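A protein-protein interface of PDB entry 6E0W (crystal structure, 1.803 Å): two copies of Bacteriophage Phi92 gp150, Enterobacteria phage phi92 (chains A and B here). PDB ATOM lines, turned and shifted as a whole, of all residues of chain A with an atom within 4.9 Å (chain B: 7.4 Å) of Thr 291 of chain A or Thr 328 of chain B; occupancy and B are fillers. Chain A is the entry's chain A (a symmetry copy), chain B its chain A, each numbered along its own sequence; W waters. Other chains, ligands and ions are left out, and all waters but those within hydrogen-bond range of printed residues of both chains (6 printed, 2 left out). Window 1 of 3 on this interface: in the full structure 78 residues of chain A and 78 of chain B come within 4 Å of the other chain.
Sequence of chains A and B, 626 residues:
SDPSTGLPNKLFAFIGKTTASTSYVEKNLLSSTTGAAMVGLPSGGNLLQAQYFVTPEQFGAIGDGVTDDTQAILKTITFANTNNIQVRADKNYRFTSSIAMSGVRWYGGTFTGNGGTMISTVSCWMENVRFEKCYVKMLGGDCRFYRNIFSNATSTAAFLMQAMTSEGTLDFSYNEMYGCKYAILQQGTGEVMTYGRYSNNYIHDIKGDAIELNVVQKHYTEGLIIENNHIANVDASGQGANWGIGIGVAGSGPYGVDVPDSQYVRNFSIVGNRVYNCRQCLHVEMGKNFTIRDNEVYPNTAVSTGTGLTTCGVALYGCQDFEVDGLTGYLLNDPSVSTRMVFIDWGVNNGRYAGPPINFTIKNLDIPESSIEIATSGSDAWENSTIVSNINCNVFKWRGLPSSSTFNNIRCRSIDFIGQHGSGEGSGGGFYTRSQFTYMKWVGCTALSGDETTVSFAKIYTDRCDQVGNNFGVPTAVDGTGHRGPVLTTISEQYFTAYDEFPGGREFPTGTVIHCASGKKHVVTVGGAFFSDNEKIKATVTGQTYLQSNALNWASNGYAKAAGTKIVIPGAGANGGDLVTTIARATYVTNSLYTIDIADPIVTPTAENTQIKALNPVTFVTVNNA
The side-chain carboxylate of Asp 294 of chain B lies within salt-bridge range of the guanidinium group of Arg 293 of chain A (3.9 Å).
The backbone NH (N) of Thr 328 of chain B is in hydrogen-bond range of the backbone carbonyl oxygen (O) of Asn 295 of chain B.
The backbone NH (N) of Val 297 of chain B is in hydrogen-bond range of the backbone carbonyl oxygen (O) of Thr 328 of chain B.
The backbone carbonyl oxygen (O) of Val 297 of chain B lies within hydrogen-bond range of the backbone NH (N) of Tyr 330 of chain B, 3.2 Å away.
N of Thr 291 of chain A is in hydrogen-bond range of O of Phe 268 of chain A.
The backbone carbonyl oxygen of Ile 270 of chain A is in hydrogen-bond range of the backbone NH of Arg 293 of chain A (2.8 Å).
The side-chain carboxylate of Glu 323 of chain A is in hydrogen-bond range of the side-chain hydroxyl of Thr 291 of chain A.
CG of Asn 289 of chain A touches CE2 of Tyr 330 of chain B (3.9 Å).
Thr 328 of chain B touches Thr 291 of chain A (CG2 to OG1, 3.7 Å).
Thr 328 of chain B touches Glu 323 of chain A.
CG of Glu 323 of chain A touches CG of Asp 366 of chain B, 3.7 Å away.
Of the printed residues of chain B, Asn 289 of chain A touches Tyr 330 (3.9 Å).
Of the printed residues of chain B, Thr 291 of chain A touches Thr 328.
Of the printed residues of chain A, Asp 294 of chain B touches Arg 293.
Thr 328 of chain B touches just these residues of chain A: Thr 291 (3.7 Å) and Glu 323 (3.7 Å).
Gly 329 of chain B touches none of the printed residues of chain A.
Of the printed residues of chain A, Asp 366 of chain B touches Glu 323 (3.7 Å).
The nearest residue of chain B that does not touch Thr 291 of chain A is Glu 296 of chain B (6.1 Å).
Of the 21 printed residues of chain B, 4 touch a printed residue of chain A.
Printed residues of chain B that touch a printed residue of chain A: Asp 294, Thr 328, Tyr 330 and Asp 366.
Hydrophobic or aromatic side chains of chain B that line the printed part of chain A: Tyr 330.
Of the 10 printed residues of chain A, 4 touch a printed residue of chain B.
Printed residues of chain A that touch a printed residue of chain B: Asn 289, Thr 291, Arg 293 and Glu 323.
Among the printed residues, 5 pairs touch across the chains.
Among the printed residues, Asp or Glu carboxylates within 4 Å of a Lys or Arg side-chain nitrogen of the other chain: Arg 293 of chain A with Asp 294 of chain B.
No position is printed for both chains.
Water W4 lies within hydrogen-bond range of the side-chain carboxylate (OE2) of Glu 296 of chain B and the side-chain hydroxyl (OG) of Ser 269 of chain A.
Water W1 lies within hydrogen-bond range of the side-chain carboxylate (OE1) of Glu 323 of chain A and the side-chain carboxylate (OD2) of Asp 366 of chain B.
Water W5 lies within hydrogen-bond range of the side-chain hydroxyl (OG1) of Thr 328 of chain B (2.7 Å), the side-chain carboxylate (OE2) of Glu 296 of chain B (3.0 Å) and the side-chain hydroxyl (OG1) of Thr 291 of chain A (3.2 Å).
Water W3 lies within hydrogen-bond range of OH of Tyr 298 of chain B and O of Asn 289 of chain A.
Water W2 bridges O of Phe 268 of chain A (2.8 Å) and OE1 of Glu 296 of chain B (2.9 Å).
Water W6 lies within hydrogen-bond range of the backbone carbonyl oxygen of Asn 295 of chain B (2.9 Å), the side-chain hydroxyl of Thr 328 of chain B (3.0 Å) and the guanidinium group of Arg 293 of chain A (3.3 Å).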
ATOM      1  N   PHE A 268      -0.546 -21.465 -31.166  1.00  0.00           N
ATOM      2  CA  PHE A 268      -1.448 -20.345 -31.377  1.00  0.00           C
ATOM      3  C   PHE A 268      -2.311 -20.122 -30.131  1.00  0.00           C
ATOM      4  O   PHE A 268      -2.358 -20.948 -29.215  1.00  0.00           O
ATOM      5  CB  PHE A 268      -2.326 -20.539 -32.636  1.00  0.00           C
ATOM      6  CG  PHE A 268      -3.300 -21.717 -32.603  1.00  0.00           C
ATOM      7  CD1 PHE A 268      -2.945 -22.966 -33.099  1.00  0.00           C
ATOM      8  CD2 PHE A 268      -4.623 -21.525 -32.170  1.00  0.00           C
ATOM      9  CE1 PHE A 268      -3.870 -24.046 -33.088  1.00  0.00           C
ATOM     10  CE2 PHE A 268      -5.542 -22.584 -32.139  1.00  0.00           C
ATOM     11  CZ  PHE A 268      -5.174 -23.846 -32.634  1.00  0.00           C
ATOM     12  N   SER A 269      -3.024 -19.000 -30.108  1.00  0.00           N
ATOM     13  CA  SER A 269      -3.950 -18.789 -29.000  1.00  0.00           C
ATOM     14  C   SER A 269      -5.210 -18.068 -29.460  1.00  0.00           C
ATOM     15  O   SER A 269      -5.167 -17.221 -30.362  1.00  0.00           O
ATOM     16  CB  SER A 269      -3.272 -18.026 -27.876  1.00  0.00           C
ATOM     17  OG  SER A 269      -2.606 -16.876 -28.384  1.00  0.00           O
ATOM     18  N   ILE A 270      -6.337 -18.431 -28.820  1.00  0.00           N
ATOM     19  CA  ILE A 270      -7.665 -17.881 -29.085  1.00  0.00           C
ATOM     20  C   ILE A 270      -8.184 -17.461 -27.723  1.00  0.00           C
ATOM     21  O   ILE A 270      -8.559 -18.319 -26.907  1.00  0.00           O
ATOM     22  CB  ILE A 270      -8.601 -18.901 -29.740  1.00  0.00           C
ATOM     23  CG1 ILE A 270      -7.986 -19.385 -31.057  1.00  0.00           C
ATOM     24  CG2 ILE A 270      -9.991 -18.304 -29.909  1.00  0.00           C
ATOM     25  CD1 ILE A 270      -8.790 -20.444 -31.773  1.00  0.00           C
ATOM     26  N   VAL A 271      -8.155 -16.162 -27.448  1.00  0.00           N
ATOM     27  CA  VAL A 271      -8.236 -15.641 -26.086  1.00  0.00           C
ATOM     28  C   VAL A 271      -9.229 -14.492 -26.032  1.00  0.00           C
ATOM     29  O   VAL A 271      -9.095 -13.532 -26.796  1.00  0.00           O
ATOM     30  CB  VAL A 271      -6.860 -15.137 -25.620  1.00  0.00           C
ATOM     31  CG1 VAL A 271      -6.978 -14.516 -24.195  1.00  0.00           C
ATOM     32  CG2 VAL A 271      -5.839 -16.272 -25.636  1.00  0.00           C
ATOM     33  N   ASN A 289      -0.400 -27.949 -29.309  1.00  0.00           N
ATOM     34  CA  ASN A 289       0.313 -26.947 -28.496  1.00  0.00           C
ATOM     35  C   ASN A 289      -0.357 -25.585 -28.565  1.00  0.00           C
ATOM     36  O   ASN A 289       0.303 -24.583 -28.851  1.00  0.00           O
ATOM     37  CB  ASN A 289       1.780 -26.827 -28.934  1.00  0.00           C
ATOM     38  CG  ASN A 289       2.544 -28.052 -28.618  1.00  0.00           C
ATOM     39  OD1 ASN A 289       2.426 -28.589 -27.533  1.00  0.00           O
ATOM     40  ND2 ASN A 289       3.324 -28.530 -29.566  1.00  0.00           N
ATOM     41  N   PHE A 290      -1.666 -25.548 -28.248  1.00  0.00           N
ATOM     42  CA  PHE A 290      -2.446 -24.322 -28.350  1.00  0.00           C
ATOM     43  C   PHE A 290      -3.326 -24.169 -27.111  1.00  0.00           C
ATOM     44  O   PHE A 290      -3.502 -25.099 -26.315  1.00  0.00           O
ATOM     45  CB  PHE A 290      -3.329 -24.300 -29.635  1.00  0.00           C
ATOM     46  CG  PHE A 290      -4.435 -25.302 -29.633  1.00  0.00           C
ATOM     47  CD1 PHE A 290      -5.697 -24.973 -29.138  1.00  0.00           C
ATOM     48  CD2 PHE A 290      -4.240 -26.564 -30.197  1.00  0.00           C
ATOM     49  CE1 PHE A 290      -6.743 -25.889 -29.136  1.00  0.00           C
ATOM     50  CE2 PHE A 290      -5.267 -27.475 -30.206  1.00  0.00           C
ATOM     51  CZ  PHE A 290      -6.546 -27.130 -29.658  1.00  0.00           C
ATOM     52  N   THR A 291      -3.873 -22.974 -26.964  1.00  0.00           N
ATOM     53  CA  THR A 291      -4.683 -22.607 -25.806  1.00  0.00           C
ATOM     54  C   THR A 291      -5.891 -21.831 -26.278  1.00  0.00           C
ATOM     55  O   THR A 291      -5.759 -20.916 -27.098  1.00  0.00           O
ATOM     56  CB  THR A 291      -3.896 -21.732 -24.817  1.00  0.00           C
ATOM     57  OG1 THR A 291      -2.751 -22.450 -24.366  1.00  0.00           O
ATOM     58  CG2 THR A 291      -4.759 -21.368 -23.597  1.00  0.00           C
ATOM     59  N   ILE A 292      -7.054 -22.177 -25.720  1.00  0.00           N
ATOM     60  CA  ILE A 292      -8.312 -21.489 -25.979  1.00  0.00           C
ATOM     61  C   ILE A 292      -8.777 -20.965 -24.622  1.00  0.00           C
ATOM     62  O   ILE A 292      -9.197 -21.754 -23.768  1.00  0.00           O
ATOM     63  CB  ILE A 292      -9.349 -22.413 -26.624  1.00  0.00           C
ATOM     64  CG1 ILE A 292      -8.759 -22.973 -27.941  1.00  0.00           C
ATOM     65  CG2 ILE A 292     -10.649 -21.621 -26.903  1.00  0.00           C
ATOM     66  CD1 ILE A 292      -9.677 -23.787 -28.745  1.00  0.00           C
ATOM     67  N   ARG A 293      -8.648 -19.657 -24.393  1.00  0.00           N
ATOM     68  CA  ARG A 293      -8.748 -19.113 -23.031  1.00  0.00           C
ATOM     69  C   ARG A 293      -9.774 -17.994 -22.921  1.00  0.00           C
ATOM     70  O   ARG A 293      -9.718 -17.031 -23.684  1.00  0.00           O
ATOM     71  CB  ARG A 293      -7.395 -18.572 -22.582  1.00  0.00           C
ATOM     72  CG  ARG A 293      -7.458 -17.884 -21.207  1.00  0.00           C
ATOM     73  CD  ARG A 293      -6.024 -17.609 -20.654  1.00  0.00           C
ATOM     74  NE  ARG A 293      -5.497 -16.398 -21.237  1.00  0.00           N
ATOM     75  CZ  ARG A 293      -4.402 -16.354 -21.981  1.00  0.00           C
ATOM     76  NH1 ARG A 293      -3.693 -17.465 -22.194  1.00  0.00           N
ATOM     77  NH2 ARG A 293      -3.999 -15.197 -22.488  1.00  0.00           N
ATOM     78  N   GLU A 323      -5.177 -26.685 -24.098  1.00  0.00           N
ATOM     79  CA  GLU A 323      -6.107 -26.446 -22.987  1.00  0.00           C
ATOM     80  C   GLU A 323      -7.290 -25.635 -23.483  1.00  0.00           C
ATOM     81  O   GLU A 323      -7.153 -24.800 -24.385  1.00  0.00           O
ATOM     82  CB  GLU A 323      -5.489 -25.645 -21.814  1.00  0.00           C
ATOM     83  CG  GLU A 323      -4.188 -26.117 -21.331  1.00  0.00           C
ATOM     84  CD  GLU A 323      -3.092 -25.442 -22.131  1.00  0.00           C
ATOM     85  OE1 GLU A 323      -3.291 -24.254 -22.485  1.00  0.00           O
ATOM     86  OE2 GLU A 323      -2.105 -26.102 -22.471  1.00  0.00           O
ATOM     87  N   ASN B 273       1.258 -11.494 -21.949  1.00  0.00           N
ATOM     88  CA  ASN B 273       2.326 -11.306 -22.923  1.00  0.00           C
ATOM     89  C   ASN B 273       2.750 -12.638 -23.543  1.00  0.00           C
ATOM     90  O   ASN B 273       2.512 -13.708 -22.993  1.00  0.00           O
ATOM     91  CB  ASN B 273       3.534 -10.643 -22.274  1.00  0.00           C
ATOM     92  CG  ASN B 273       3.176  -9.319 -21.632  1.00  0.00           C
ATOM     93  OD1 ASN B 273       3.077  -8.317 -22.319  1.00  0.00           O
ATOM     94  ND2 ASN B 273       2.884  -9.335 -20.317  1.00  0.00           N
ATOM     95  N   VAL B 275       6.308 -14.336 -25.133  1.00  0.00           N
ATOM     96  CA  VAL B 275       7.755 -14.162 -25.235  1.00  0.00           C
ATOM     97  C   VAL B 275       8.339 -15.432 -25.839  1.00  0.00           C
ATOM     98  O   VAL B 275       8.395 -16.473 -25.167  1.00  0.00           O
ATOM     99  CB  VAL B 275       8.395 -13.856 -23.875  1.00  0.00           C
ATOM    100  CG1 VAL B 275       9.876 -13.471 -24.089  1.00  0.00           C
ATOM    101  CG2 VAL B 275       7.657 -12.755 -23.168  1.00  0.00           C
ATOM    102  N   ASP B 294      -1.238 -15.141 -16.946  1.00  0.00           N
ATOM    103  CA  ASP B 294      -1.600 -15.589 -18.310  1.00  0.00           C
ATOM    104  C   ASP B 294      -0.570 -15.176 -19.365  1.00  0.00           C
ATOM    105  O   ASP B 294      -0.904 -14.645 -20.427  1.00  0.00           O
ATOM    106  CB  ASP B 294      -2.984 -15.082 -18.692  1.00  0.00           C
ATOM    107  CG  ASP B 294      -4.086 -15.765 -17.895  1.00  0.00           C
ATOM    108  OD1 ASP B 294      -3.866 -16.947 -17.531  1.00  0.00           O
ATOM    109  OD2 ASP B 294      -5.118 -15.091 -17.593  1.00  0.00           O
ATOM    110  N   ASN B 295       0.693 -15.461 -19.093  1.00  0.00           N
ATOM    111  CA  ASN B 295       1.737 -15.235 -20.085  1.00  0.00           C
ATOM    112  C   ASN B 295       2.095 -16.543 -20.782  1.00  0.00           C
ATOM    113  O   ASN B 295       1.966 -17.620 -20.205  1.00  0.00           O
ATOM    114  CB  ASN B 295       2.972 -14.637 -19.414  1.00  0.00           C
ATOM    115  CG  ASN B 295       2.697 -13.245 -18.818  1.00  0.00           C
ATOM    116  OD1 ASN B 295       2.682 -12.234 -19.538  1.00  0.00           O
ATOM    117  ND2 ASN B 295       2.408 -13.199 -17.528  1.00  0.00           N
ATOM    118  N   GLU B 296       2.609 -16.433 -22.004  1.00  0.00           N
ATOM    119  CA  GLU B 296       2.993 -17.574 -22.822  1.00  0.00           C
ATOM    120  C   GLU B 296       4.454 -17.401 -23.181  1.00  0.00           C
ATOM    121  O   GLU B 296       4.810 -16.395 -23.816  1.00  0.00           O
ATOM    122  CB  GLU B 296       2.141 -17.624 -24.097  1.00  0.00           C
ATOM    123  CG  GLU B 296       2.509 -18.761 -25.079  1.00  0.00           C
ATOM    124  CD  GLU B 296       1.665 -18.720 -26.364  1.00  0.00           C
ATOM    125  OE1 GLU B 296       1.892 -19.521 -27.311  1.00  0.00           O
ATOM    126  OE2 GLU B 296       0.751 -17.878 -26.431  1.00  0.00           O
ATOM    127  N   VAL B 297       5.299 -18.380 -22.814  1.00  0.00           N
ATOM    128  CA  VAL B 297       6.744 -18.181 -22.923  1.00  0.00           C
ATOM    129  C   VAL B 297       7.442 -19.408 -23.512  1.00  0.00           C
ATOM    130  O   VAL B 297       7.084 -20.553 -23.223  1.00  0.00           O
ATOM    131  CB  VAL B 297       7.363 -17.813 -21.540  1.00  0.00           C
ATOM    132  CG1 VAL B 297       6.784 -16.474 -20.988  1.00  0.00           C
ATOM    133  CG2 VAL B 297       7.156 -18.949 -20.530  1.00  0.00           C
ATOM    134  N   TYR B 298       8.519 -19.159 -24.278  1.00  0.00           N
ATOM    135  CA  TYR B 298       9.292 -20.215 -24.928  1.00  0.00           C
ATOM    136  C   TYR B 298      10.773 -19.921 -24.709  1.00  0.00           C
ATOM    137  O   TYR B 298      11.392 -19.272 -25.547  1.00  0.00           O
ATOM    138  CB  TYR B 298       8.977 -20.268 -26.415  1.00  0.00           C
ATOM    139  CG  TYR B 298       7.515 -20.571 -26.683  1.00  0.00           C
ATOM    140  CD1 TYR B 298       7.080 -21.874 -26.794  1.00  0.00           C
ATOM    141  CD2 TYR B 298       6.605 -19.551 -26.861  1.00  0.00           C
ATOM    142  CE1 TYR B 298       5.713 -22.180 -27.068  1.00  0.00           C
ATOM    143  CE2 TYR B 298       5.243 -19.827 -27.148  1.00  0.00           C
ATOM    144  CZ  TYR B 298       4.811 -21.132 -27.220  1.00  0.00           C
ATOM    145  OH  TYR B 298       3.485 -21.405 -27.472  1.00  0.00           O
ATOM    146  N   PRO B 299      11.335 -20.324 -23.577  1.00  0.00           N
ATOM    147  CA  PRO B 299      12.774 -20.082 -23.313  1.00  0.00           C
ATOM    148  C   PRO B 299      13.663 -20.916 -24.227  1.00  0.00           C
ATOM    149  O   PRO B 299      13.248 -21.920 -24.815  1.00  0.00           O
ATOM    150  CB  PRO B 299      12.950 -20.529 -21.866  1.00  0.00           C
ATOM    151  CG  PRO B 299      11.512 -20.555 -21.278  1.00  0.00           C
ATOM    152  CD  PRO B 299      10.678 -21.003 -22.461  1.00  0.00           C
ATOM    153  N   GLY B 313      11.317 -19.540 -17.930  1.00  0.00           N
ATOM    154  CA  GLY B 313      10.177 -18.742 -18.380  1.00  0.00           C
ATOM    155  C   GLY B 313       9.896 -17.619 -17.404  1.00  0.00           C
ATOM    156  O   GLY B 313       9.612 -16.482 -17.799  1.00  0.00           O
ATOM    157  N   GLY B 326      -1.316 -18.705 -14.206  1.00  0.00           N
ATOM    158  CA  GLY B 326      -1.477 -18.986 -15.615  1.00  0.00           C
ATOM    159  C   GLY B 326      -0.162 -18.853 -16.373  1.00  0.00           C
ATOM    160  O   GLY B 326       0.442 -17.786 -16.401  1.00  0.00           O
ATOM    161  N   LEU B 327       0.294 -19.936 -16.995  1.00  0.00           N
ATOM    162  CA  LEU B 327       1.533 -19.925 -17.773  1.00  0.00           C
ATOM    163  C   LEU B 327       1.436 -21.067 -18.754  1.00  0.00           C
ATOM    164  O   LEU B 327       1.026 -22.161 -18.362  1.00  0.00           O
ATOM    165  CB  LEU B 327       2.787 -20.143 -16.938  1.00  0.00           C
ATOM    166  CG  LEU B 327       4.148 -19.918 -17.604  1.00  0.00           C
ATOM    167  CD1 LEU B 327       4.368 -18.457 -17.951  1.00  0.00           C
ATOM    168  CD2 LEU B 327       5.308 -20.362 -16.659  1.00  0.00           C
ATOM    169  N   THR B 328       1.831 -20.808 -19.997  1.00  0.00           N
ATOM    170  CA  THR B 328       1.854 -21.803 -21.070  1.00  0.00           C
ATOM    171  C   THR B 328       3.156 -21.617 -21.836  1.00  0.00           C
ATOM    172  O   THR B 328       3.872 -20.639 -21.625  1.00  0.00           O
ATOM    173  CB  THR B 328       0.677 -21.640 -22.034  1.00  0.00           C
ATOM    174  OG1 THR B 328       0.706 -20.313 -22.581  1.00  0.00           O
ATOM    175  CG2 THR B 328      -0.675 -21.872 -21.306  1.00  0.00           C
ATOM    176  N   GLY B 329       3.443 -22.552 -22.758  1.00  0.00           N
ATOM    177  CA  GLY B 329       4.699 -22.578 -23.500  1.00  0.00           C
ATOM    178  C   GLY B 329       5.574 -23.731 -23.058  1.00  0.00           C
ATOM    179  O   GLY B 329       5.165 -24.601 -22.284  1.00  0.00           O
ATOM    180  N   TYR B 330       6.799 -23.750 -23.594  1.00  0.00           N
ATOM    181  CA  TYR B 330       7.743 -24.823 -23.317  1.00  0.00           C
ATOM    182  C   TYR B 330       9.113 -24.347 -23.802  1.00  0.00           C
ATOM    183  O   TYR B 330       9.220 -23.333 -24.495  1.00  0.00           O
ATOM    184  CB  TYR B 330       7.330 -26.137 -23.994  1.00  0.00           C
ATOM    185  CG  TYR B 330       7.062 -25.992 -25.459  1.00  0.00           C
ATOM    186  CD1 TYR B 330       8.103 -25.937 -26.399  1.00  0.00           C
ATOM    187  CD2 TYR B 330       5.746 -25.933 -25.932  1.00  0.00           C
ATOM    188  CE1 TYR B 330       7.835 -25.806 -27.784  1.00  0.00           C
ATOM    189  CE2 TYR B 330       5.479 -25.845 -27.316  1.00  0.00           C
ATOM    190  CZ  TYR B 330       6.516 -25.760 -28.229  1.00  0.00           C
ATOM    191  OH  TYR B 330       6.214 -25.640 -29.588  1.00  0.00           O
ATOM    192  N   MET B 341      11.404 -23.970 -16.210  1.00  0.00           N
ATOM    193  CA  MET B 341      10.395 -23.004 -16.634  1.00  0.00           C
ATOM    194  C   MET B 341      10.011 -22.009 -15.546  1.00  0.00           C
ATOM    195  O   MET B 341       9.754 -20.843 -15.844  1.00  0.00           O
ATOM    196  CB  MET B 341       9.115 -23.736 -17.066  1.00  0.00           C
ATOM    197  CG  MET B 341       8.000 -22.819 -17.553  1.00  0.00           C
ATOM    198  SD  MET B 341       8.532 -21.987 -19.052  1.00  0.00           S
ATOM    199  CE  MET B 341       8.098 -23.152 -20.313  1.00  0.00           C
ATOM    200  N   ASN B 364      -2.408 -22.395 -11.695  1.00  0.00           N
ATOM    201  CA  ASN B 364      -2.980 -22.452 -13.052  1.00  0.00           C
ATOM    202  C   ASN B 364      -1.896 -22.570 -14.112  1.00  0.00           C
ATOM    203  O   ASN B 364      -2.050 -22.031 -15.194  1.00  0.00           O
ATOM    204  CB  ASN B 364      -3.851 -21.223 -13.354  1.00  0.00           C
ATOM    205  CG  ASN B 364      -4.997 -21.104 -12.382  1.00  0.00           C
ATOM    206  OD1 ASN B 364      -5.490 -22.122 -11.919  1.00  0.00           O
ATOM    207  ND2 ASN B 364      -5.392 -19.885 -12.027  1.00  0.00           N
ATOM    208  N   LEU B 365      -0.785 -23.251 -13.820  1.00  0.00           N
ATOM    209  CA  LEU B 365       0.282 -23.408 -14.796  1.00  0.00           C
ATOM    210  C   LEU B 365       0.058 -24.643 -15.666  1.00  0.00           C
ATOM    211  O   LEU B 365      -0.087 -25.757 -15.152  1.00  0.00           O
ATOM    212  CB  LEU B 365       1.638 -23.513 -14.098  1.00  0.00           C
ATOM    213  CG  LEU B 365       1.938 -22.464 -13.023  1.00  0.00           C
ATOM    214  CD1 LEU B 365       3.397 -22.671 -12.563  1.00  0.00           C
ATOM    215  CD2 LEU B 365       1.705 -21.034 -13.518  1.00  0.00           C
ATOM    216  N   ASP B 366       0.132 -24.457 -16.984  1.00  0.00           N
ATOM    217  CA  ASP B 366      -0.081 -25.546 -17.928  1.00  0.00           C
ATOM    218  C   ASP B 366       1.234 -25.750 -18.681  1.00  0.00           C
ATOM    219  O   ASP B 366       1.381 -25.301 -19.835  1.00  0.00           O
ATOM    220  CB  ASP B 366      -1.203 -25.186 -18.856  1.00  0.00           C
ATOM    221  CG  ASP B 366      -2.571 -25.095 -18.131  1.00  0.00           C
ATOM    222  OD1 ASP B 366      -3.014 -26.154 -17.616  1.00  0.00           O
ATOM    223  OD2 ASP B 366      -3.156 -23.955 -18.047  1.00  0.00           O
ATOM    224  N   ILE B 367       2.186 -26.407 -18.016  1.00  0.00           N
ATOM    225  CA  ILE B 367       3.531 -26.555 -18.575  1.00  0.00           C
ATOM    226  C   ILE B 367       4.004 -27.999 -18.396  1.00  0.00           C
ATOM    227  O   ILE B 367       5.052 -28.236 -17.780  1.00  0.00           O
ATOM    228  CB  ILE B 367       4.512 -25.555 -17.928  1.00  0.00           C
ATOM    229  CG1 ILE B 367       4.362 -25.592 -16.412  1.00  0.00           C
ATOM    230  CG2 ILE B 367       4.226 -24.115 -18.432  1.00  0.00           C
ATOM    231  CD1 ILE B 367       5.610 -24.921 -15.634  1.00  0.00           C
ATOM    232  N   PRO B 368       3.278 -28.986 -18.934  1.00  0.00           N
ATOM    233  CA  PRO B 368       3.559 -30.388 -18.571  1.00  0.00           C
ATOM    234  C   PRO B 368       4.994 -30.812 -18.892  1.00  0.00           C
ATOM    235  O   PRO B 368       5.528 -31.708 -18.220  1.00  0.00           O
ATOM    236  CB  PRO B 368       2.541 -31.189 -19.433  1.00  0.00           C
ATOM    237  CG  PRO B 368       2.070 -30.232 -20.553  1.00  0.00           C
ATOM    238  CD  PRO B 368       2.102 -28.859 -19.824  1.00  0.00           C
ATOM    239  N   GLU B 369       5.604 -30.225 -19.926  1.00  0.00           N
ATOM    240  CA  GLU B 369       6.959 -30.654 -20.350  1.00  0.00           C
ATOM    241  C   GLU B 369       8.063 -30.082 -19.464  1.00  0.00           C
ATOM    242  O   GLU B 369       9.233 -30.528 -19.566  1.00  0.00           O
ATOM    243  CB  GLU B 369       7.230 -30.197 -21.784  1.00  0.00           C
ATOM    244  CG  GLU B 369       6.141 -30.595 -22.817  1.00  0.00           C
ATOM    245  CD  GLU B 369       5.009 -29.534 -22.994  1.00  0.00           C
ATOM    246  OE1 GLU B 369       4.335 -29.591 -24.052  1.00  0.00           O
ATOM    247  OE2 GLU B 369       4.763 -28.656 -22.113  1.00  0.00           O
HETATM  248  O   HOH W   1      -4.186 -22.900 -20.360  1.00  0.00           O
HETATM  249  O   HOH W   2      -0.297 -21.377 -27.403  1.00  0.00           O
HETATM  250  O   HOH W   3       2.444 -23.871 -27.113  1.00  0.00           O
HETATM  251  O   HOH W   4       0.000 -17.882 -28.967  1.00  0.00           O
HETATM  252  O   HOH W   5      -0.784 -19.935 -24.793  1.00  0.00           O
HETATM  253  O   HOH W   6      -0.814 -18.328 -20.871  1.00  0.00           O
